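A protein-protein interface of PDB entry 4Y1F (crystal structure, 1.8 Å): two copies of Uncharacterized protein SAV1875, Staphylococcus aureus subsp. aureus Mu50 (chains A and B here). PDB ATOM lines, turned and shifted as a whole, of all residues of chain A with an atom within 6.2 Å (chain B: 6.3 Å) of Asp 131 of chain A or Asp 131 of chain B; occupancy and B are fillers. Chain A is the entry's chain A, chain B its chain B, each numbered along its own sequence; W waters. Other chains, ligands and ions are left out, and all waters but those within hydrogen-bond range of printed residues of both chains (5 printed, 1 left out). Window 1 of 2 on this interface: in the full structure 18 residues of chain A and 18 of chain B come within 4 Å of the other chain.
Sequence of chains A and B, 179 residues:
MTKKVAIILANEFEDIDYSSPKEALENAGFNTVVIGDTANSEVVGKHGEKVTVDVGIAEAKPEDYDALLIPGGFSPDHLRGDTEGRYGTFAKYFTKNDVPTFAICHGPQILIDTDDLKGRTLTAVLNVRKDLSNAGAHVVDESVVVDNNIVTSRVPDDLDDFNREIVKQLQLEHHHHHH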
ATOM      1  N   ARG A  80     -21.120  -9.055  -2.805  1.00  0.00           N
ATOM      2  CA  ARG A  80     -20.341  -9.673  -3.879  1.00  0.00           C
ATOM      3  C   ARG A  80     -18.866  -9.353  -3.759  1.00  0.00           C
ATOM      4  O   ARG A  80     -18.047  -9.919  -4.481  1.00  0.00           O
ATOM      5  CB  ARG A  80     -20.862  -9.216  -5.251  1.00  0.00           C
ATOM      6  CG  ARG A  80     -22.284  -9.687  -5.513  1.00  0.00           C
ATOM      7  CD  ARG A  80     -22.780  -9.165  -6.849  1.00  0.00           C
ATOM      8  NE  ARG A  80     -22.345  -9.991  -7.981  1.00  0.00           N
ATOM      9  CZ  ARG A  80     -22.333  -9.577  -9.249  1.00  0.00           C
ATOM     10  NH1 ARG A  80     -22.652  -8.318  -9.562  1.00  0.00           N
ATOM     11  NH2 ARG A  80     -22.007 -10.438 -10.213  1.00  0.00           N
ATOM     12  N   GLN A 109     -28.448  -8.891  -8.592  1.00  0.00           N
ATOM     13  CA  GLN A 109     -26.979  -9.009  -8.708  1.00  0.00           C
ATOM     14  C   GLN A 109     -26.401 -10.248  -8.052  1.00  0.00           C
ATOM     15  O   GLN A 109     -25.490 -10.875  -8.590  1.00  0.00           O
ATOM     16  CB  GLN A 109     -26.285  -7.772  -8.129  1.00  0.00           C
ATOM     17  CG  GLN A 109     -26.416  -6.548  -9.017  1.00  0.00           C
ATOM     18  CD  GLN A 109     -25.672  -5.345  -8.462  1.00  0.00           C
ATOM     19  OE1 GLN A 109     -25.867  -4.953  -7.302  1.00  0.00           O
ATOM     20  NE2 GLN A 109     -24.763  -4.780  -9.280  1.00  0.00           N
ATOM     21  N   ILE A 112     -26.617 -13.502 -10.040  1.00  0.00           N
ATOM     22  CA  ILE A 112     -25.620 -13.706 -11.094  1.00  0.00           C
ATOM     23  C   ILE A 112     -24.519 -14.621 -10.574  1.00  0.00           C
ATOM     24  O   ILE A 112     -24.011 -15.484 -11.298  1.00  0.00           O
ATOM     25  CB  ILE A 112     -25.002 -12.354 -11.530  1.00  0.00           C
ATOM     26  CG1 ILE A 112     -26.078 -11.474 -12.175  1.00  0.00           C
ATOM     27  CG2 ILE A 112     -23.822 -12.598 -12.479  1.00  0.00           C
ATOM     28  CD1 ILE A 112     -25.591 -10.068 -12.479  1.00  0.00           C
ATOM     29  N   ASP A 113     -24.181 -14.478  -9.290  1.00  0.00           N
ATOM     30  CA  ASP A 113     -23.090 -15.284  -8.723  1.00  0.00           C
ATOM     31  C   ASP A 113     -23.445 -16.768  -8.510  1.00  0.00           C
ATOM     32  O   ASP A 113     -22.561 -17.594  -8.252  1.00  0.00           O
ATOM     33  CB  ASP A 113     -22.591 -14.649  -7.418  1.00  0.00           C
ATOM     34  CG  ASP A 113     -21.857 -13.336  -7.669  1.00  0.00           C
ATOM     35  OD1 ASP A 113     -21.543 -13.065  -8.849  1.00  0.00           O
ATOM     36  OD2 ASP A 113     -21.623 -12.568  -6.705  1.00  0.00           O
ATOM     37  N   ASN A 127     -30.162  -0.209 -13.759  1.00  0.00           N
ATOM     38  CA  ASN A 127     -28.687  -0.228 -13.608  1.00  0.00           C
ATOM     39  C   ASN A 127     -28.073  -1.614 -13.808  1.00  0.00           C
ATOM     40  O   ASN A 127     -26.854  -1.745 -13.905  1.00  0.00           O
ATOM     41  CB  ASN A 127     -28.262   0.250 -12.201  1.00  0.00           C
ATOM     42  CG  ASN A 127     -28.938   1.532 -11.775  1.00  0.00           C
ATOM     43  OD1 ASN A 127     -28.284   2.436 -11.213  1.00  0.00           O
ATOM     44  ND2 ASN A 127     -30.232   1.648 -12.056  1.00  0.00           N
ATOM     45  N   VAL A 128     -28.879  -2.654 -13.608  1.00  0.00           N
ATOM     46  CA  VAL A 128     -28.349  -4.007 -13.432  1.00  0.00           C
ATOM     47  C   VAL A 128     -28.854  -4.931 -14.552  1.00  0.00           C
ATOM     48  O   VAL A 128     -28.400  -6.059 -14.692  1.00  0.00           O
ATOM     49  CB  VAL A 128     -28.787  -4.563 -12.061  1.00  0.00           C
ATOM     50  CG1 VAL A 128     -28.897  -6.076 -12.073  1.00  0.00           C
ATOM     51  CG2 VAL A 128     -27.843  -4.068 -10.968  1.00  0.00           C
ATOM     52  N   ARG A 129     -29.796  -4.446 -15.361  1.00  0.00           N
ATOM     53  CA  ARG A 129     -30.399  -5.291 -16.384  1.00  0.00           C
ATOM     54  C   ARG A 129     -29.423  -5.857 -17.401  1.00  0.00           C
ATOM     55  O   ARG A 129     -29.552  -6.996 -17.826  1.00  0.00           O
ATOM     56  CB  ARG A 129     -31.532  -4.547 -17.091  1.00  0.00           C
ATOM     57  CG  ARG A 129     -32.768  -4.492 -16.219  1.00  0.00           C
ATOM     58  CD  ARG A 129     -33.906  -3.818 -16.971  1.00  0.00           C
ATOM     59  NE  ARG A 129     -34.773  -3.219 -15.984  1.00  0.00           N
ATOM     60  CZ  ARG A 129     -35.559  -2.182 -16.201  1.00  0.00           C
ATOM     61  NH1 ARG A 129     -35.636  -1.622 -17.412  1.00  0.00           N
ATOM     62  NH2 ARG A 129     -36.247  -1.696 -15.186  1.00  0.00           N
ATOM     63  N   LYS A 130     -28.460  -5.052 -17.817  1.00  0.00           N
ATOM     64  CA  LYS A 130     -27.479  -5.532 -18.771  1.00  0.00           C
ATOM     65  C   LYS A 130     -26.639  -6.677 -18.186  1.00  0.00           C
ATOM     66  O   LYS A 130     -26.343  -7.663 -18.880  1.00  0.00           O
ATOM     67  CB  LYS A 130     -26.604  -4.380 -19.273  1.00  0.00           C
ATOM     68  CG  LYS A 130     -25.339  -4.806 -20.010  1.00  0.00           C
ATOM     69  CD  LYS A 130     -25.633  -5.423 -21.370  1.00  0.00           C
ATOM     70  CE  LYS A 130     -26.746  -4.681 -22.099  1.00  0.00           C
ATOM     71  NZ  LYS A 130     -26.402  -4.473 -23.534  1.00  0.00           N
ATOM     72  N   ASP A 131     -26.282  -6.564 -16.913  1.00  0.00           N
ATOM     73  CA  ASP A 131     -25.454  -7.592 -16.279  1.00  0.00           C
ATOM     74  C   ASP A 131     -26.267  -8.880 -16.162  1.00  0.00           C
ATOM     75  O   ASP A 131     -25.763  -9.963 -16.403  1.00  0.00           O
ATOM     76  CB  ASP A 131     -24.936  -7.112 -14.906  1.00  0.00           C
ATOM     77  CG  ASP A 131     -23.958  -5.928 -15.032  1.00  0.00           C
ATOM     78  OD1 ASP A 131     -23.351  -5.756 -16.127  1.00  0.00           O
ATOM     79  OD2 ASP A 131     -23.707  -5.228 -14.022  1.00  0.00           O
ATOM     80  N   LEU A 132     -27.559  -8.743 -15.890  1.00  0.00           N
ATOM     81  CA  LEU A 132     -28.426  -9.903 -15.793  1.00  0.00           C
ATOM     82  C   LEU A 132     -28.563 -10.613 -17.144  1.00  0.00           C
ATOM     83  O   LEU A 132     -28.491 -11.852 -17.231  1.00  0.00           O
ATOM     84  CB  LEU A 132     -29.801  -9.446 -15.320  1.00  0.00           C
ATOM     85  CG  LEU A 132     -30.522 -10.101 -14.163  1.00  0.00           C
ATOM     86  CD1 LEU A 132     -29.583 -10.578 -13.057  1.00  0.00           C
ATOM     87  CD2 LEU A 132     -31.567  -9.098 -13.667  1.00  0.00           C
ATOM     88  N   SER A 133     -28.673  -9.838 -18.209  1.00  0.00           N
ATOM     89  CA  SER A 133     -28.778 -10.438 -19.537  1.00  0.00           C
ATOM     90  C   SER A 133     -27.472 -11.103 -19.977  1.00  0.00           C
ATOM     91  O   SER A 133     -27.486 -12.190 -20.536  1.00  0.00           O
ATOM     92  CB  SER A 133     -29.179  -9.381 -20.563  1.00  0.00           C
ATOM     93  OG  SER A 133     -29.295  -9.993 -21.846  1.00  0.00           O
ATOM     94  N   ASN A 134     -26.341 -10.507 -19.642  1.00  0.00           N
ATOM     95  CA  ASN A 134     -25.033 -11.133 -19.892  1.00  0.00           C
ATOM     96  C   ASN A 134     -24.833 -12.419 -19.097  1.00  0.00           C
ATOM     97  O   ASN A 134     -24.046 -13.292 -19.495  1.00  0.00           O
ATOM     98  CB  ASN A 134     -23.891 -10.162 -19.540  1.00  0.00           C
ATOM     99  CG  ASN A 134     -23.748  -9.039 -20.546  1.00  0.00           C
ATOM    100  OD1 ASN A 134     -24.252  -9.119 -21.667  1.00  0.00           O
ATOM    101  ND2 ASN A 134     -23.042  -8.006 -20.163  1.00  0.00           N
ATOM    102  N   ALA A 135     -25.560 -12.536 -17.987  1.00  0.00           N
ATOM    103  CA  ALA A 135     -25.507 -13.753 -17.179  1.00  0.00           C
ATOM    104  C   ALA A 135     -26.438 -14.843 -17.699  1.00  0.00           C
ATOM    105  O   ALA A 135     -26.505 -15.931 -17.123  1.00  0.00           O
ATOM    106  CB  ALA A 135     -25.797 -13.457 -15.714  1.00  0.00           C
ATOM    107  N   GLY A 136     -27.155 -14.553 -18.780  1.00  0.00           N
ATOM    108  CA  GLY A 136     -27.951 -15.565 -19.429  1.00  0.00           C
ATOM    109  C   GLY A 136     -29.444 -15.435 -19.204  1.00  0.00           C
ATOM    110  O   GLY A 136     -30.212 -16.231 -19.752  1.00  0.00           O
ATOM    111  N   ARG B  80     -24.943   4.251 -14.781  1.00  0.00           N
ATOM    112  CA  ARG B  80     -25.644   3.198 -15.503  1.00  0.00           C
ATOM    113  C   ARG B  80     -27.140   3.236 -15.287  1.00  0.00           C
ATOM    114  O   ARG B  80     -27.878   2.508 -15.963  1.00  0.00           O
ATOM    115  CB  ARG B  80     -25.121   1.819 -15.106  1.00  0.00           C
ATOM    116  CG  ARG B  80     -23.666   1.595 -15.446  1.00  0.00           C
ATOM    117  CD  ARG B  80     -23.251   0.179 -15.072  1.00  0.00           C
ATOM    118  NE  ARG B  80     -23.617  -0.801 -16.101  1.00  0.00           N
ATOM    119  CZ  ARG B  80     -23.622  -2.114 -15.902  1.00  0.00           C
ATOM    120  NH1 ARG B  80     -23.345  -2.576 -14.689  1.00  0.00           N
ATOM    121  NH2 ARG B  80     -23.708  -2.957 -16.939  1.00  0.00           N
ATOM    122  N   GLN B 109     -17.411  -1.039 -14.902  1.00  0.00           N
ATOM    123  CA  GLN B 109     -18.837  -1.347 -15.127  1.00  0.00           C
ATOM    124  C   GLN B 109     -19.424  -0.565 -16.302  1.00  0.00           C
ATOM    125  O   GLN B 109     -20.309  -1.044 -17.014  1.00  0.00           O
ATOM    126  CB  GLN B 109     -19.652  -1.011 -13.870  1.00  0.00           C
ATOM    127  CG  GLN B 109     -19.585  -2.098 -12.815  1.00  0.00           C
ATOM    128  CD  GLN B 109     -20.365  -1.742 -11.564  1.00  0.00           C
ATOM    129  OE1 GLN B 109     -20.217  -0.648 -11.009  1.00  0.00           O
ATOM    130  NE2 GLN B 109     -21.197  -2.678 -11.103  1.00  0.00           N
ATOM    131  N   ILE B 112     -19.069  -2.079 -19.665  1.00  0.00           N
ATOM    132  CA  ILE B 112     -19.992  -3.161 -19.974  1.00  0.00           C
ATOM    133  C   ILE B 112     -21.112  -2.690 -20.899  1.00  0.00           C
ATOM    134  O   ILE B 112     -21.466  -3.375 -21.875  1.00  0.00           O
ATOM    135  CB  ILE B 112     -20.545  -3.798 -18.688  1.00  0.00           C
ATOM    136  CG1 ILE B 112     -19.403  -4.523 -17.962  1.00  0.00           C
ATOM    137  CG2 ILE B 112     -21.670  -4.776 -19.003  1.00  0.00           C
ATOM    138  CD1 ILE B 112     -19.816  -5.126 -16.625  1.00  0.00           C
ATOM    139  N   ASP B 113     -21.533  -1.451 -20.709  1.00  0.00           N
ATOM    140  CA  ASP B 113     -22.663  -0.917 -21.454  1.00  0.00           C
ATOM    141  C   ASP B 113     -22.300  -0.546 -22.881  1.00  0.00           C
ATOM    142  O   ASP B 113     -23.194  -0.380 -23.727  1.00  0.00           O
ATOM    143  CB  ASP B 113     -23.266   0.280 -20.733  1.00  0.00           C
ATOM    144  CG  ASP B 113     -24.032  -0.129 -19.495  1.00  0.00           C
ATOM    145  OD1 ASP B 113     -24.321  -1.339 -19.366  1.00  0.00           O
ATOM    146  OD2 ASP B 113     -24.366   0.752 -18.675  1.00  0.00           O
ATOM    147  N   ASN B 127     -15.665  -7.082  -6.762  1.00  0.00           N
ATOM    148  CA  ASN B 127     -17.136  -7.014  -6.790  1.00  0.00           C
ATOM    149  C   ASN B 127     -17.678  -7.096  -8.215  1.00  0.00           C
ATOM    150  O   ASN B 127     -18.867  -7.369  -8.398  1.00  0.00           O
ATOM    151  CB  ASN B 127     -17.668  -5.714  -6.131  1.00  0.00           C
ATOM    152  CG  ASN B 127     -17.087  -5.456  -4.749  1.00  0.00           C
ATOM    153  OD1 ASN B 127     -17.823  -5.183  -3.771  1.00  0.00           O
ATOM    154  ND2 ASN B 127     -15.772  -5.603  -4.635  1.00  0.00           N
ATOM    155  N   VAL B 128     -16.903  -6.624  -9.199  1.00  0.00           N
ATOM    156  CA  VAL B 128     -17.458  -6.492 -10.567  1.00  0.00           C
ATOM    157  C   VAL B 128     -16.827  -7.439 -11.595  1.00  0.00           C
ATOM    158  O   VAL B 128     -17.225  -7.474 -12.776  1.00  0.00           O
ATOM    159  CB  VAL B 128     -17.369  -5.032 -11.071  1.00  0.00           C
ATOM    160  CG1 VAL B 128     -17.985  -4.078 -10.063  1.00  0.00           C
ATOM    161  CG2 VAL B 128     -15.923  -4.651 -11.323  1.00  0.00           C
ATOM    162  N   ARG B 129     -15.923  -8.292 -11.135  1.00  0.00           N
ATOM    163  CA  ARG B 129     -15.190  -9.158 -12.037  1.00  0.00           C
ATOM    164  C   ARG B 129     -16.097 -10.148 -12.762  1.00  0.00           C
ATOM    165  O   ARG B 129     -15.956 -10.383 -13.958  1.00  0.00           O
ATOM    166  CB  ARG B 129     -14.075  -9.892 -11.280  1.00  0.00           C
ATOM    167  CG  ARG B 129     -12.951  -8.950 -10.937  1.00  0.00           C
ATOM    168  CD  ARG B 129     -11.709  -9.667 -10.438  1.00  0.00           C
ATOM    169  NE  ARG B 129     -10.848  -8.676  -9.802  1.00  0.00           N
ATOM    170  CZ  ARG B 129     -10.031  -8.925  -8.785  1.00  0.00           C
ATOM    171  NH1 ARG B 129      -9.968 -10.143  -8.264  1.00  0.00           N
ATOM    172  NH2 ARG B 129      -9.481  -7.905  -8.140  1.00  0.00           N
ATOM    173  N   LYS B 130     -17.053 -10.718 -12.042  1.00  0.00           N
ATOM    174  CA  LYS B 130     -17.937 -11.669 -12.685  1.00  0.00           C
ATOM    175  C   LYS B 130     -18.682 -10.996 -13.828  1.00  0.00           C
ATOM    176  O   LYS B 130     -18.847 -11.603 -14.911  1.00  0.00           O
ATOM    177  CB  LYS B 130     -18.934 -12.239 -11.673  1.00  0.00           C
ATOM    178  CG  LYS B 130     -19.910 -13.221 -12.301  1.00  0.00           C
ATOM    179  CD  LYS B 130     -19.195 -14.488 -12.717  1.00  0.00           C
ATOM    180  CE  LYS B 130     -19.198 -15.481 -11.558  1.00  0.00           C
ATOM    181  NZ  LYS B 130     -19.376 -16.849 -12.104  1.00  0.00           N
ATOM    182  N   ASP B 131     -19.228  -9.807 -13.572  1.00  0.00           N
ATOM    183  CA  ASP B 131     -19.974  -9.098 -14.610  1.00  0.00           C
ATOM    184  C   ASP B 131     -19.088  -8.771 -15.821  1.00  0.00           C
ATOM    185  O   ASP B 131     -19.548  -8.861 -16.957  1.00  0.00           O
ATOM    186  CB  ASP B 131     -20.674  -7.836 -14.074  1.00  0.00           C
ATOM    187  CG  ASP B 131     -21.687  -8.156 -12.944  1.00  0.00           C
ATOM    188  OD1 ASP B 131     -22.235  -9.284 -12.927  1.00  0.00           O
ATOM    189  OD2 ASP B 131     -21.865  -7.322 -12.025  1.00  0.00           O
ATOM    190  N   LEU B 132     -17.824  -8.424 -15.584  1.00  0.00           N
ATOM    191  CA  LEU B 132     -16.909  -8.226 -16.727  1.00  0.00           C
ATOM    192  C   LEU B 132     -16.654  -9.506 -17.538  1.00  0.00           C
ATOM    193  O   LEU B 132     -16.693  -9.488 -18.767  1.00  0.00           O
ATOM    194  CB  LEU B 132     -15.586  -7.599 -16.283  1.00  0.00           C
ATOM    195  CG  LEU B 132     -15.696  -6.198 -15.680  1.00  0.00           C
ATOM    196  CD1 LEU B 132     -14.382  -5.931 -14.966  1.00  0.00           C
ATOM    197  CD2 LEU B 132     -15.874  -5.197 -16.815  1.00  0.00           C
ATOM    198  N   SER B 133     -16.484 -10.639 -16.851  1.00  0.00           N
ATOM    199  CA  SER B 133     -16.335 -11.911 -17.524  1.00  0.00           C
ATOM    200  C   SER B 133     -17.578 -12.230 -18.343  1.00  0.00           C
ATOM    201  O   SER B 133     -17.485 -12.755 -19.458  1.00  0.00           O
ATOM    202  CB  SER B 133     -16.055 -13.030 -16.497  1.00  0.00           C
ATOM    203  OG  SER B 133     -14.838 -12.768 -15.811  1.00  0.00           O
ATOM    204  N   ASN B 134     -18.755 -11.967 -17.779  1.00  0.00           N
ATOM    205  CA  ASN B 134     -19.988 -12.301 -18.479  1.00  0.00           C
ATOM    206  C   ASN B 134     -20.173 -11.419 -19.733  1.00  0.00           C
ATOM    207  O   ASN B 134     -20.907 -11.783 -20.677  1.00  0.00           O
ATOM    208  CB  ASN B 134     -21.205 -12.155 -17.557  1.00  0.00           C
ATOM    209  CG  ASN B 134     -21.391 -13.369 -16.641  1.00  0.00           C
ATOM    210  OD1 ASN B 134     -20.811 -14.433 -16.874  1.00  0.00           O
ATOM    211  ND2 ASN B 134     -22.215 -13.217 -15.617  1.00  0.00           N
ATOM    212  N   ALA B 135     -19.500 -10.266 -19.717  1.00  0.00           N
ATOM    213  CA  ALA B 135     -19.502  -9.325 -20.853  1.00  0.00           C
ATOM    214  C   ALA B 135     -18.485  -9.756 -21.896  1.00  0.00           C
ATOM    215  O   ALA B 135     -18.392  -9.166 -22.981  1.00  0.00           O
ATOM    216  CB  ALA B 135     -19.201  -7.904 -20.375  1.00  0.00           C
ATOM    217  N   GLY B 136     -17.802 -10.852 -21.618  1.00  0.00           N
ATOM    218  CA  GLY B 136     -16.880 -11.420 -22.572  1.00  0.00           C
ATOM    219  C   GLY B 136     -15.431 -11.030 -22.401  1.00  0.00           C
ATOM    220  O   GLY B 136     -14.579 -11.462 -23.197  1.00  0.00           O
HETATM  221  O   HOH W   1     -23.380 -15.615 -14.046  1.00  0.00           O
HETATM  222  O   HOH W   2     -21.852  -6.056 -22.296  1.00  0.00           O
HETATM  223  O   HOH W   3     -21.478  -5.966  -7.894  1.00  0.00           O
HETATM  224  O   HOH W   4     -22.128  -8.174 -17.320  1.00  0.00           O
HETATM  225  O   HOH W   5     -23.152 -10.397 -15.553  1.00  0.00           O
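Of the 14 printed residues of chain A, 8 touch a printed residue of chain B. Printed residues of chain A that touch a printed residue of chain B: Arg 80, Ile 112, Asp 113, Asn 127, Lys 130, Asp 131, Asn 134 and Ala 135.
Arg 80 of chain A touches Lys 130 of chain B, and with the chains exchanged Lys 130 of chain A touches Arg 80 of chain B. Arg 80 of chain A touches Asp 131 of chain B, and with the chains exchanged Asp 131 of chain A touches Arg 80 of chain B. Ile 112 of chain A touches Lys 130 of chain B, and with the chains exchanged Lys 130 of chain A touches Ile 112 of chain B. Asp 113 of chain A touches Lys 130 of chain B, and with the chains exchanged Lys 130 of chain A touches Asp 113 of chain B. Of the 18 pairs that touch across the chains among the printed residues, 18 have their exchanged pair printed and touching as well.
NH1 of Arg 80 of chain A lies within salt-bridge range of OD2 of Asp 131 of chain B (2.8 Å). The side-chain carboxylate of Asp 131 of chain A lies within salt-bridge range of the guanidinium group of Arg 80 of chain B. OD2 of Asp 131 of chain A lies close to OD2 of Asp 131 of chain B (3.4 Å).
Water W4 lies within hydrogen-bond range of the backbone carbonyl oxygen of Asp 131 of chain B (2.7 Å), the side-chain carboxylate of Asp 131 of chain A (3.0 Å) and the side-chain amide nitrogen of Asn 134 of chain A (3.0 Å). Water W2 lies within hydrogen-bond range of O of Ile 112 of chain B and ND2 of Asn 134 of chain A. Water W5 lies within hydrogen-bond range of the backbone carbonyl oxygen of Asp 131 of chain A (2.8 Å), the side-chain amide nitrogen of Asn 134 of chain B (3.0 Å) and the side-chain carboxylate of Asp 131 of chain B (3.0 Å). Water W1 lies within hydrogen-bond range of O of Ile 112 of chain A (2.8 Å) and ND2 of Asn 134 of chain B (3.1 Å). Water W3 lies within hydrogen-bond range of the backbone carbonyl oxygen of Asn 127 of chain B (3.0 Å) and the guanidinium group of Arg 80 of chain A (3.1 Å).
Printed residues of chain B within 4 Å of Asp 131 of chain A: Arg 80, Ile 112 and Asp 131. Asp 131 of chain B touches three residues of chain A. Of the printed residues of chain A, Asn 127 of chain B touches Arg 80 (3.8 Å). Printed residues of chain B within 4 Å of Ala 135 of chain A: Asn 134 (3.6 Å). Printed residues of chain A within 4 Å of Ile 112 of chain B: Lys 130, Asp 131 and Asn 134. Ser 133 of chain B touches none of the printed residues of chain A. Gly 136 of chain B touches none of the printed residues of chain A. The nearest residue of chain B that does not touch Asp 131 of chain A is Gln 109 of chain B (4.6 Å). The nearest residue of chain A that does not touch Asp 131 of chain B is Gln 109 of chain A (4.7 Å). The nearest printed residue of chain B that does not touch Asn 127 of chain A is Asp 113 of chain B (5.9 Å).
Arg 80 of chain A touches Lys 130 of chain B. CG2 of Ile 112 of chain A touches CG of Lys 130 of chain B, 3.97 Å away. Ile 112 of chain A touches Asp 131 of chain B (CD1 to OD1, 3.5 Å). CG2 of Ile 112 of chain A touches ND2 of Asn 134 of chain B, 3.6 Å away. Asn 127 of chain A touches Arg 80 of chain B. Lys 130 of chain A touches Ile 112 of chain B. Ile 112 of chain B touches Asp 131 of chain A (CG2 to OD1, 3.5 Å). Asn 134 of chain A touches Ile 112 of chain B. Asn 134 of chain B touches Asn 134 of chain A (O to CB, 3.6 Å). ND2 of Asn 134 of chain B touches CB of Ala 135 of chain A, at 3.6 Å.
The guanidinium group (NE) of Arg 80 of chain A lies within hydrogen-bond range of the backbone carbonyl oxygen (O) of Gln 109 of chain A (3.3 Å). The guanidinium group of Arg 80 of chain A lies within salt-bridge range of the side-chain carboxylate of Asp 113 of chain A (3.0 Å). The backbone carbonyl oxygen of Gln 109 of chain B is in hydrogen-bond range of the guanidinium group of Arg 80 of chain B (3.4 Å). The side-chain carboxylate of Asp 113 of chain B lies within salt-bridge range of the guanidinium group of Arg 80 of chain B, at 3.0 Å.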
